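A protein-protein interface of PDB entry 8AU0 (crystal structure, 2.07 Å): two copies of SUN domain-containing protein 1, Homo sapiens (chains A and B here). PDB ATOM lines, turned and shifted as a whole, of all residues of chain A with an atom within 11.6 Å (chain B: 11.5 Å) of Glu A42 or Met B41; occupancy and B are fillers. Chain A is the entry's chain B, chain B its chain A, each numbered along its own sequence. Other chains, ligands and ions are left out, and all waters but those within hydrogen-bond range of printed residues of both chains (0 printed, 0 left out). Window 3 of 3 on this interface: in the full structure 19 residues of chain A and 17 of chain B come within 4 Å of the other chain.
Of chain A, only Val A38 (3.6 Å), Met A41 (3.5 Å) and Glu A42 (3.7 Å) come within 4 Å of Met B41.
Of chain B, only Arg B37 (3.3 Å) comes within 4 Å of Asp A39.
Of chain A, only Gln A35 (3.1 Å), Val A38 (3.8 Å), Asp A39 (3.3 Å) and Glu A42 (2.6 Å) come within 4 Å of Arg B37.
Printed residues of chain A within 4 Å of Val B38: Val A38.
No residue of chain A comes within 4 Å of Gln B40.
Printed residues of chain A within 4 Å of Leu B34: Leu A34 (3.7 Å), Gln A35 (3.8 Å) and Val A38 (3.8 Å).
Of the printed residues of chain B, Leu A34 touches Leu B34.
Of the printed residues of chain B, Gln A35 touches Leu B34 (3.8 Å) and Arg B37 (3.1 Å).
Gln A32 touches none of the printed residues of chain B.
The nearest residue of chain A that does not touch Met B41 is Asp A39 (6.4 Å).
The nearest printed residue of chain B that does not touch Gln A35 is Leu B31 (7.3 Å).
Leu B34 touches Leu A34 (CD2 to CB, 3.7 Å).
Gln A35 touches Leu B34.
CB of Val A38 touches CD1 of Leu B34 (3.8 Å).
Arg B37 touches Val A38 (NE to CG1, 3.8 Å).
Val B38 touches Val A38.
CE of Met B41 touches CG1 of Val A38 (3.6 Å).
Met A41 touches Met B41.
Glu A42 touches Met B41 (CG to SD, 3.7 Å).
Hydrophobic or aromatic side chains of chain A within 4 Å of the printed part of chain B: Leu A34, Val A38 and Met A41.
Of the 11 printed residues of chain B, 4 touch a printed residue of chain A.
Printed residues of chain B that touch a printed residue of chain A: Leu B34, Arg B37, Val B38 and Met B41.
Hydrophobic or aromatic side chains of chain B that line the printed part of chain A: Leu B34, Val B38 and Met B41.
Among the printed residues, Asp or Glu carboxylates within 4 Å of a Lys or Arg side-chain nitrogen of the other chain: Asp A39 with Arg B37 and Glu A42 with Arg B37.
The side-chain carboxylate (OE1) of Glu A42 lies within salt-bridge range of the guanidinium group (NH1) of Arg B37, 2.6 Å away.
NH1 of Arg B37 lies within salt-bridge range of OD1 of Asp A39, 3.3 Å away.
NH2 of Arg B37 is in hydrogen-bond range of O of Gln A35.
Gln A35 touches Leu B34, but with the chains exchanged Leu A34 does not touch Gln B35 (7.7 Å).
Gln A35 touches Arg B37, but with the chains exchanged Arg A37 does not touch Gln B35 (11.2 Å).
Val B38 touches its own counterpart, Val A38.
Asp A39 touches Arg B37, but with the chains exchanged Arg A37 does not touch Asp B39 (11.9 Å).
Of the 11 pairs that touch across the chains among the printed residues, 3 have their exchanged pair printed and touching as well.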
ATOM      1  N   GLN A  32     -24.304 -17.536   1.567  1.00  0.00           N
ATOM      2  CA  GLN A  32     -25.371 -18.515   1.372  1.00  0.00           C
ATOM      3  C   GLN A  32     -25.768 -18.624  -0.098  1.00  0.00           C
ATOM      4  O   GLN A  32     -26.112 -19.713  -0.576  1.00  0.00           O
ATOM      5  CB  GLN A  32     -26.576 -18.176   2.270  1.00  0.00           C
ATOM      6  CG  GLN A  32     -26.414 -18.668   3.753  1.00  0.00           C
ATOM      7  CD  GLN A  32     -27.368 -18.024   4.741  1.00  0.00           C
ATOM      8  OE1 GLN A  32     -28.116 -17.097   4.394  1.00  0.00           O
ATOM      9  NE2 GLN A  32     -27.342 -18.504   5.987  1.00  0.00           N
ATOM     10  N   LYS A  33     -25.688 -17.529  -0.851  1.00  0.00           N
ATOM     11  CA  LYS A  33     -25.973 -17.634  -2.271  1.00  0.00           C
ATOM     12  C   LYS A  33     -24.844 -18.332  -2.997  1.00  0.00           C
ATOM     13  O   LYS A  33     -25.093 -19.112  -3.923  1.00  0.00           O
ATOM     14  CB  LYS A  33     -26.212 -16.267  -2.891  1.00  0.00           C
ATOM     15  CG  LYS A  33     -27.406 -15.554  -2.305  1.00  0.00           C
ATOM     16  CD  LYS A  33     -27.553 -14.188  -2.952  1.00  0.00           C
ATOM     17  CE  LYS A  33     -27.744 -14.315  -4.447  1.00  0.00           C
ATOM     18  NZ  LYS A  33     -28.409 -13.098  -4.993  1.00  0.00           N
ATOM     19  N   LEU A  34     -23.596 -18.080  -2.592  1.00  0.00           N
ATOM     20  CA  LEU A  34     -22.489 -18.816  -3.197  1.00  0.00           C
ATOM     21  C   LEU A  34     -22.592 -20.313  -2.923  1.00  0.00           C
ATOM     22  O   LEU A  34     -22.335 -21.131  -3.818  1.00  0.00           O
ATOM     23  CB  LEU A  34     -21.155 -18.288  -2.684  1.00  0.00           C
ATOM     24  CG  LEU A  34     -20.334 -17.498  -3.698  1.00  0.00           C
ATOM     25  CD1 LEU A  34     -19.026 -17.209  -3.032  1.00  0.00           C
ATOM     26  CD2 LEU A  34     -20.138 -18.222  -5.044  1.00  0.00           C
ATOM     27  N   GLN A  35     -22.963 -20.682  -1.693  1.00  0.00           N
ATOM     28  CA  GLN A  35     -23.106 -22.087  -1.320  1.00  0.00           C
ATOM     29  C   GLN A  35     -24.082 -22.794  -2.231  1.00  0.00           C
ATOM     30  O   GLN A  35     -23.866 -23.943  -2.624  1.00  0.00           O
ATOM     31  CB  GLN A  35     -23.613 -22.207   0.111  1.00  0.00           C
ATOM     32  CG  GLN A  35     -22.572 -22.156   1.183  1.00  0.00           C
ATOM     33  CD  GLN A  35     -23.166 -22.572   2.495  1.00  0.00           C
ATOM     34  OE1 GLN A  35     -23.476 -21.735   3.342  1.00  0.00           O
ATOM     35  NE2 GLN A  35     -23.365 -23.878   2.661  1.00  0.00           N
ATOM     36  N   ALA A  36     -25.209 -22.136  -2.508  1.00  0.00           N
ATOM     37  CA  ALA A  36     -26.215 -22.679  -3.410  1.00  0.00           C
ATOM     38  C   ALA A  36     -25.686 -22.769  -4.829  1.00  0.00           C
ATOM     39  O   ALA A  36     -25.828 -23.806  -5.488  1.00  0.00           O
ATOM     40  CB  ALA A  36     -27.461 -21.794  -3.378  1.00  0.00           C
ATOM     41  N   ARG A  37     -25.067 -21.685  -5.308  1.00  0.00           N
ATOM     42  CA  ARG A  37     -24.459 -21.678  -6.635  1.00  0.00           C
ATOM     43  C   ARG A  37     -23.487 -22.847  -6.807  1.00  0.00           C
ATOM     44  O   ARG A  37     -23.551 -23.582  -7.799  1.00  0.00           O
ATOM     45  CB  ARG A  37     -23.757 -20.336  -6.859  1.00  0.00           C
ATOM     46  CG  ARG A  37     -23.611 -19.852  -8.327  1.00  0.00           C
ATOM     47  CD  ARG A  37     -22.849 -18.510  -8.351  1.00  0.00           C
ATOM     48  NE  ARG A  37     -22.584 -17.946  -9.683  1.00  0.00           N
ATOM     49  CZ  ARG A  37     -21.817 -16.872  -9.898  1.00  0.00           C
ATOM     50  NH1 ARG A  37     -21.239 -16.254  -8.867  1.00  0.00           N
ATOM     51  NH2 ARG A  37     -21.633 -16.410 -11.133  1.00  0.00           N
ATOM     52  N   VAL A  38     -22.570 -23.028  -5.856  1.00  0.00           N
ATOM     53  CA  VAL A  38     -21.599 -24.120  -5.947  1.00  0.00           C
ATOM     54  C   VAL A  38     -22.289 -25.477  -5.863  1.00  0.00           C
ATOM     55  O   VAL A  38     -21.863 -26.451  -6.497  1.00  0.00           O
ATOM     56  CB  VAL A  38     -20.552 -23.940  -4.837  1.00  0.00           C
ATOM     57  CG1 VAL A  38     -19.723 -25.196  -4.681  1.00  0.00           C
ATOM     58  CG2 VAL A  38     -19.688 -22.711  -5.111  1.00  0.00           C
ATOM     59  N   ASP A  39     -23.357 -25.573  -5.065  1.00  0.00           N
ATOM     60  CA  ASP A  39     -24.109 -26.822  -4.991  1.00  0.00           C
ATOM     61  C   ASP A  39     -24.702 -27.203  -6.346  1.00  0.00           C
ATOM     62  O   ASP A  39     -24.808 -28.390  -6.664  1.00  0.00           O
ATOM     63  CB  ASP A  39     -25.219 -26.729  -3.936  1.00  0.00           C
ATOM     64  CG  ASP A  39     -25.699 -28.104  -3.504  1.00  0.00           C
ATOM     65  OD1 ASP A  39     -24.958 -28.766  -2.735  1.00  0.00           O
ATOM     66  OD2 ASP A  39     -26.784 -28.538  -3.963  1.00  0.00           O
ATOM     67  N   GLN A  40     -25.092 -26.212  -7.158  1.00  0.00           N
ATOM     68  CA  GLN A  40     -25.628 -26.481  -8.489  1.00  0.00           C
ATOM     69  C   GLN A  40     -24.541 -26.829  -9.495  1.00  0.00           C
ATOM     70  O   GLN A  40     -24.850 -27.319 -10.583  1.00  0.00           O
ATOM     71  CB  GLN A  40     -26.408 -25.276  -9.000  1.00  0.00           C
ATOM     72  CG  GLN A  40     -27.465 -24.779  -8.023  1.00  0.00           C
ATOM     73  CD  GLN A  40     -27.779 -23.300  -8.220  1.00  0.00           C
ATOM     74  OE1 GLN A  40     -27.528 -22.744  -9.294  1.00  0.00           O
ATOM     75  NE2 GLN A  40     -28.347 -22.657  -7.189  1.00  0.00           N
ATOM     76  N   MET A  41     -23.273 -26.564  -9.180  1.00  0.00           N
ATOM     77  CA  MET A  41     -22.206 -26.952 -10.095  1.00  0.00           C
ATOM     78  C   MET A  41     -21.715 -28.374  -9.852  1.00  0.00           C
ATOM     79  O   MET A  41     -20.940 -28.891 -10.665  1.00  0.00           O
ATOM     80  CB  MET A  41     -21.022 -25.984  -9.982  1.00  0.00           C
ATOM     81  CG  MET A  41     -21.300 -24.542 -10.415  1.00  0.00           C
ATOM     82  SD  MET A  41     -19.766 -23.723 -10.890  1.00  0.00           S
ATOM     83  CE  MET A  41     -18.737 -23.933  -9.442  1.00  0.00           C
ATOM     84  N   GLU A  42     -22.129 -29.000  -8.751  1.00  0.00           N
ATOM     85  CA  GLU A  42     -21.822 -30.403  -8.461  1.00  0.00           C
ATOM     86  C   GLU A  42     -23.012 -31.280  -8.809  1.00  0.00           C
ATOM     87  O   GLU A  42     -23.490 -31.271  -9.949  1.00  0.00           O
ATOM     88  CB  GLU A  42     -21.448 -30.590  -6.991  1.00  0.00           C
ATOM     89  CG  GLU A  42     -20.164 -29.846  -6.579  1.00  0.00           C
ATOM     90  CD  GLU A  42     -19.985 -29.735  -5.066  1.00  0.00           C
ATOM     91  OE1 GLU A  42     -20.945 -29.311  -4.387  1.00  0.00           O
ATOM     92  OE2 GLU A  42     -18.889 -30.069  -4.553  1.00  0.00           O
ATOM     93  N   LEU B  31     -16.505 -20.194   4.918  1.00  0.00           N
ATOM     94  CA  LEU B  31     -15.816 -19.762   3.705  1.00  0.00           C
ATOM     95  C   LEU B  31     -14.711 -20.740   3.324  1.00  0.00           C
ATOM     96  O   LEU B  31     -14.519 -21.040   2.140  1.00  0.00           O
ATOM     97  CB  LEU B  31     -15.257 -18.353   3.905  1.00  0.00           C
ATOM     98  CG  LEU B  31     -14.420 -17.733   2.784  1.00  0.00           C
ATOM     99  CD1 LEU B  31     -15.232 -17.548   1.512  1.00  0.00           C
ATOM    100  CD2 LEU B  31     -13.854 -16.407   3.249  1.00  0.00           C
ATOM    101  N   GLN B  32     -13.985 -21.259   4.318  1.00  0.00           N
ATOM    102  CA  GLN B  32     -12.915 -22.215   4.042  1.00  0.00           C
ATOM    103  C   GLN B  32     -13.468 -23.531   3.515  1.00  0.00           C
ATOM    104  O   GLN B  32     -12.837 -24.188   2.677  1.00  0.00           O
ATOM    105  CB  GLN B  32     -12.091 -22.462   5.304  1.00  0.00           C
ATOM    106  CG  GLN B  32     -11.351 -21.245   5.823  1.00  0.00           C
ATOM    107  CD  GLN B  32     -10.773 -21.479   7.203  1.00  0.00           C
ATOM    108  OE1 GLN B  32     -11.023 -22.513   7.823  1.00  0.00           O
ATOM    109  NE2 GLN B  32      -9.995 -20.522   7.693  1.00  0.00           N
ATOM    110  N   LYS B  33     -14.643 -23.941   3.997  1.00  0.00           N
ATOM    111  CA  LYS B  33     -15.238 -25.176   3.498  1.00  0.00           C
ATOM    112  C   LYS B  33     -15.735 -25.006   2.069  1.00  0.00           C
ATOM    113  O   LYS B  33     -15.553 -25.899   1.235  1.00  0.00           O
ATOM    114  CB  LYS B  33     -16.367 -25.632   4.421  1.00  0.00           C
ATOM    115  CG  LYS B  33     -15.871 -26.423   5.626  1.00  0.00           C
ATOM    116  CD  LYS B  33     -16.739 -26.206   6.856  1.00  0.00           C
ATOM    117  CE  LYS B  33     -16.156 -26.895   8.083  1.00  0.00           C
ATOM    118  NZ  LYS B  33     -16.959 -26.582   9.298  1.00  0.00           N
ATOM    119  N   LEU B  34     -16.347 -23.860   1.764  1.00  0.00           N
ATOM    120  CA  LEU B  34     -16.787 -23.613   0.395  1.00  0.00           C
ATOM    121  C   LEU B  34     -15.596 -23.454  -0.541  1.00  0.00           C
ATOM    122  O   LEU B  34     -15.621 -23.943  -1.675  1.00  0.00           O
ATOM    123  CB  LEU B  34     -17.685 -22.377   0.348  1.00  0.00           C
ATOM    124  CG  LEU B  34     -18.446 -22.155  -0.958  1.00  0.00           C
ATOM    125  CD1 LEU B  34     -19.345 -23.345  -1.265  1.00  0.00           C
ATOM    126  CD2 LEU B  34     -19.251 -20.866  -0.900  1.00  0.00           C
ATOM    127  N   GLN B  35     -14.538 -22.786  -0.080  1.00  0.00           N
ATOM    128  CA  GLN B  35     -13.349 -22.637  -0.911  1.00  0.00           C
ATOM    129  C   GLN B  35     -12.707 -23.989  -1.192  1.00  0.00           C
ATOM    130  O   GLN B  35     -12.172 -24.217  -2.284  1.00  0.00           O
ATOM    131  CB  GLN B  35     -12.349 -21.701  -0.239  1.00  0.00           C
ATOM    132  CG  GLN B  35     -11.127 -21.408  -1.084  1.00  0.00           C
ATOM    133  CD  GLN B  35     -10.284 -20.299  -0.502  1.00  0.00           C
ATOM    134  OE1 GLN B  35     -10.582 -19.776   0.570  1.00  0.00           O
ATOM    135  NE2 GLN B  35      -9.222 -19.928  -1.210  1.00  0.00           N
ATOM    136  N   ALA B  36     -12.743 -24.895  -0.215  1.00  0.00           N
ATOM    137  CA  ALA B  36     -12.238 -26.243  -0.450  1.00  0.00           C
ATOM    138  C   ALA B  36     -13.137 -27.007  -1.411  1.00  0.00           C
ATOM    139  O   ALA B  36     -12.660 -27.846  -2.183  1.00  0.00           O
ATOM    140  CB  ALA B  36     -12.112 -26.994   0.873  1.00  0.00           C
ATOM    141  N   ARG B  37     -14.443 -26.736  -1.370  1.00  0.00           N
ATOM    142  CA  ARG B  37     -15.366 -27.389  -2.289  1.00  0.00           C
ATOM    143  C   ARG B  37     -15.145 -26.908  -3.717  1.00  0.00           C
ATOM    144  O   ARG B  37     -15.300 -27.679  -4.672  1.00  0.00           O
ATOM    145  CB  ARG B  37     -16.805 -27.137  -1.842  1.00  0.00           C
ATOM    146  CG  ARG B  37     -17.828 -28.014  -2.529  1.00  0.00           C
ATOM    147  CD  ARG B  37     -19.002 -28.317  -1.606  1.00  0.00           C
ATOM    148  NE  ARG B  37     -19.896 -27.174  -1.440  1.00  0.00           N
ATOM    149  CZ  ARG B  37     -21.197 -27.192  -1.718  1.00  0.00           C
ATOM    150  NH1 ARG B  37     -21.769 -28.301  -2.164  1.00  0.00           N
ATOM    151  NH2 ARG B  37     -21.933 -26.103  -1.536  1.00  0.00           N
ATOM    152  N   VAL B  38     -14.771 -25.639  -3.882  1.00  0.00           N
ATOM    153  CA  VAL B  38     -14.471 -25.118  -5.211  1.00  0.00           C
ATOM    154  C   VAL B  38     -13.148 -25.678  -5.718  1.00  0.00           C
ATOM    155  O   VAL B  38     -13.006 -25.990  -6.906  1.00  0.00           O
ATOM    156  CB  VAL B  38     -14.477 -23.578  -5.195  1.00  0.00           C
ATOM    157  CG1 VAL B  38     -14.022 -23.028  -6.534  1.00  0.00           C
ATOM    158  CG2 VAL B  38     -15.868 -23.065  -4.858  1.00  0.00           C
ATOM    159  N   ASP B  39     -12.160 -25.828  -4.828  1.00  0.00           N
ATOM    160  CA  ASP B  39     -10.889 -26.411  -5.241  1.00  0.00           C
ATOM    161  C   ASP B  39     -11.070 -27.846  -5.724  1.00  0.00           C
ATOM    162  O   ASP B  39     -10.422 -28.273  -6.686  1.00  0.00           O
ATOM    163  CB  ASP B  39      -9.875 -26.364  -4.097  1.00  0.00           C
ATOM    164  CG  ASP B  39      -9.544 -24.952  -3.667  1.00  0.00           C
ATOM    165  OD1 ASP B  39      -9.602 -24.039  -4.515  1.00  0.00           O
ATOM    166  OD2 ASP B  39      -9.232 -24.753  -2.476  1.00  0.00           O
ATOM    167  N   GLN B  40     -11.954 -28.602  -5.070  1.00  0.00           N
ATOM    168  CA  GLN B  40     -12.139 -30.003  -5.431  1.00  0.00           C
ATOM    169  C   GLN B  40     -12.798 -30.144  -6.796  1.00  0.00           C
ATOM    170  O   GLN B  40     -12.610 -31.161  -7.474  1.00  0.00           O
ATOM    171  CB  GLN B  40     -12.959 -30.713  -4.352  1.00  0.00           C
ATOM    172  CG  GLN B  40     -12.210 -30.865  -3.024  1.00  0.00           C
ATOM    173  CD  GLN B  40     -13.122 -31.137  -1.841  1.00  0.00           C
ATOM    174  OE1 GLN B  40     -14.285 -31.505  -2.009  1.00  0.00           O
ATOM    175  NE2 GLN B  40     -12.596 -30.952  -0.634  1.00  0.00           N
ATOM    176  N   MET B  41     -13.567 -29.144  -7.215  1.00  0.00           N
ATOM    177  CA  MET B  41     -14.140 -29.136  -8.556  1.00  0.00           C
ATOM    178  C   MET B  41     -13.071 -28.773  -9.579  1.00  0.00           C
ATOM    179  O   MET B  41     -13.371 -28.556 -10.751  1.00  0.00           O
ATOM    180  CB  MET B  41     -15.307 -28.155  -8.650  1.00  0.00           C
ATOM    181  CG  MET B  41     -16.642 -28.708  -8.199  1.00  0.00           C
ATOM    182  SD  MET B  41     -17.922 -27.450  -8.346  1.00  0.00           S
ATOM    183  CE  MET B  41     -17.334 -26.252  -7.156  1.00  0.00           C
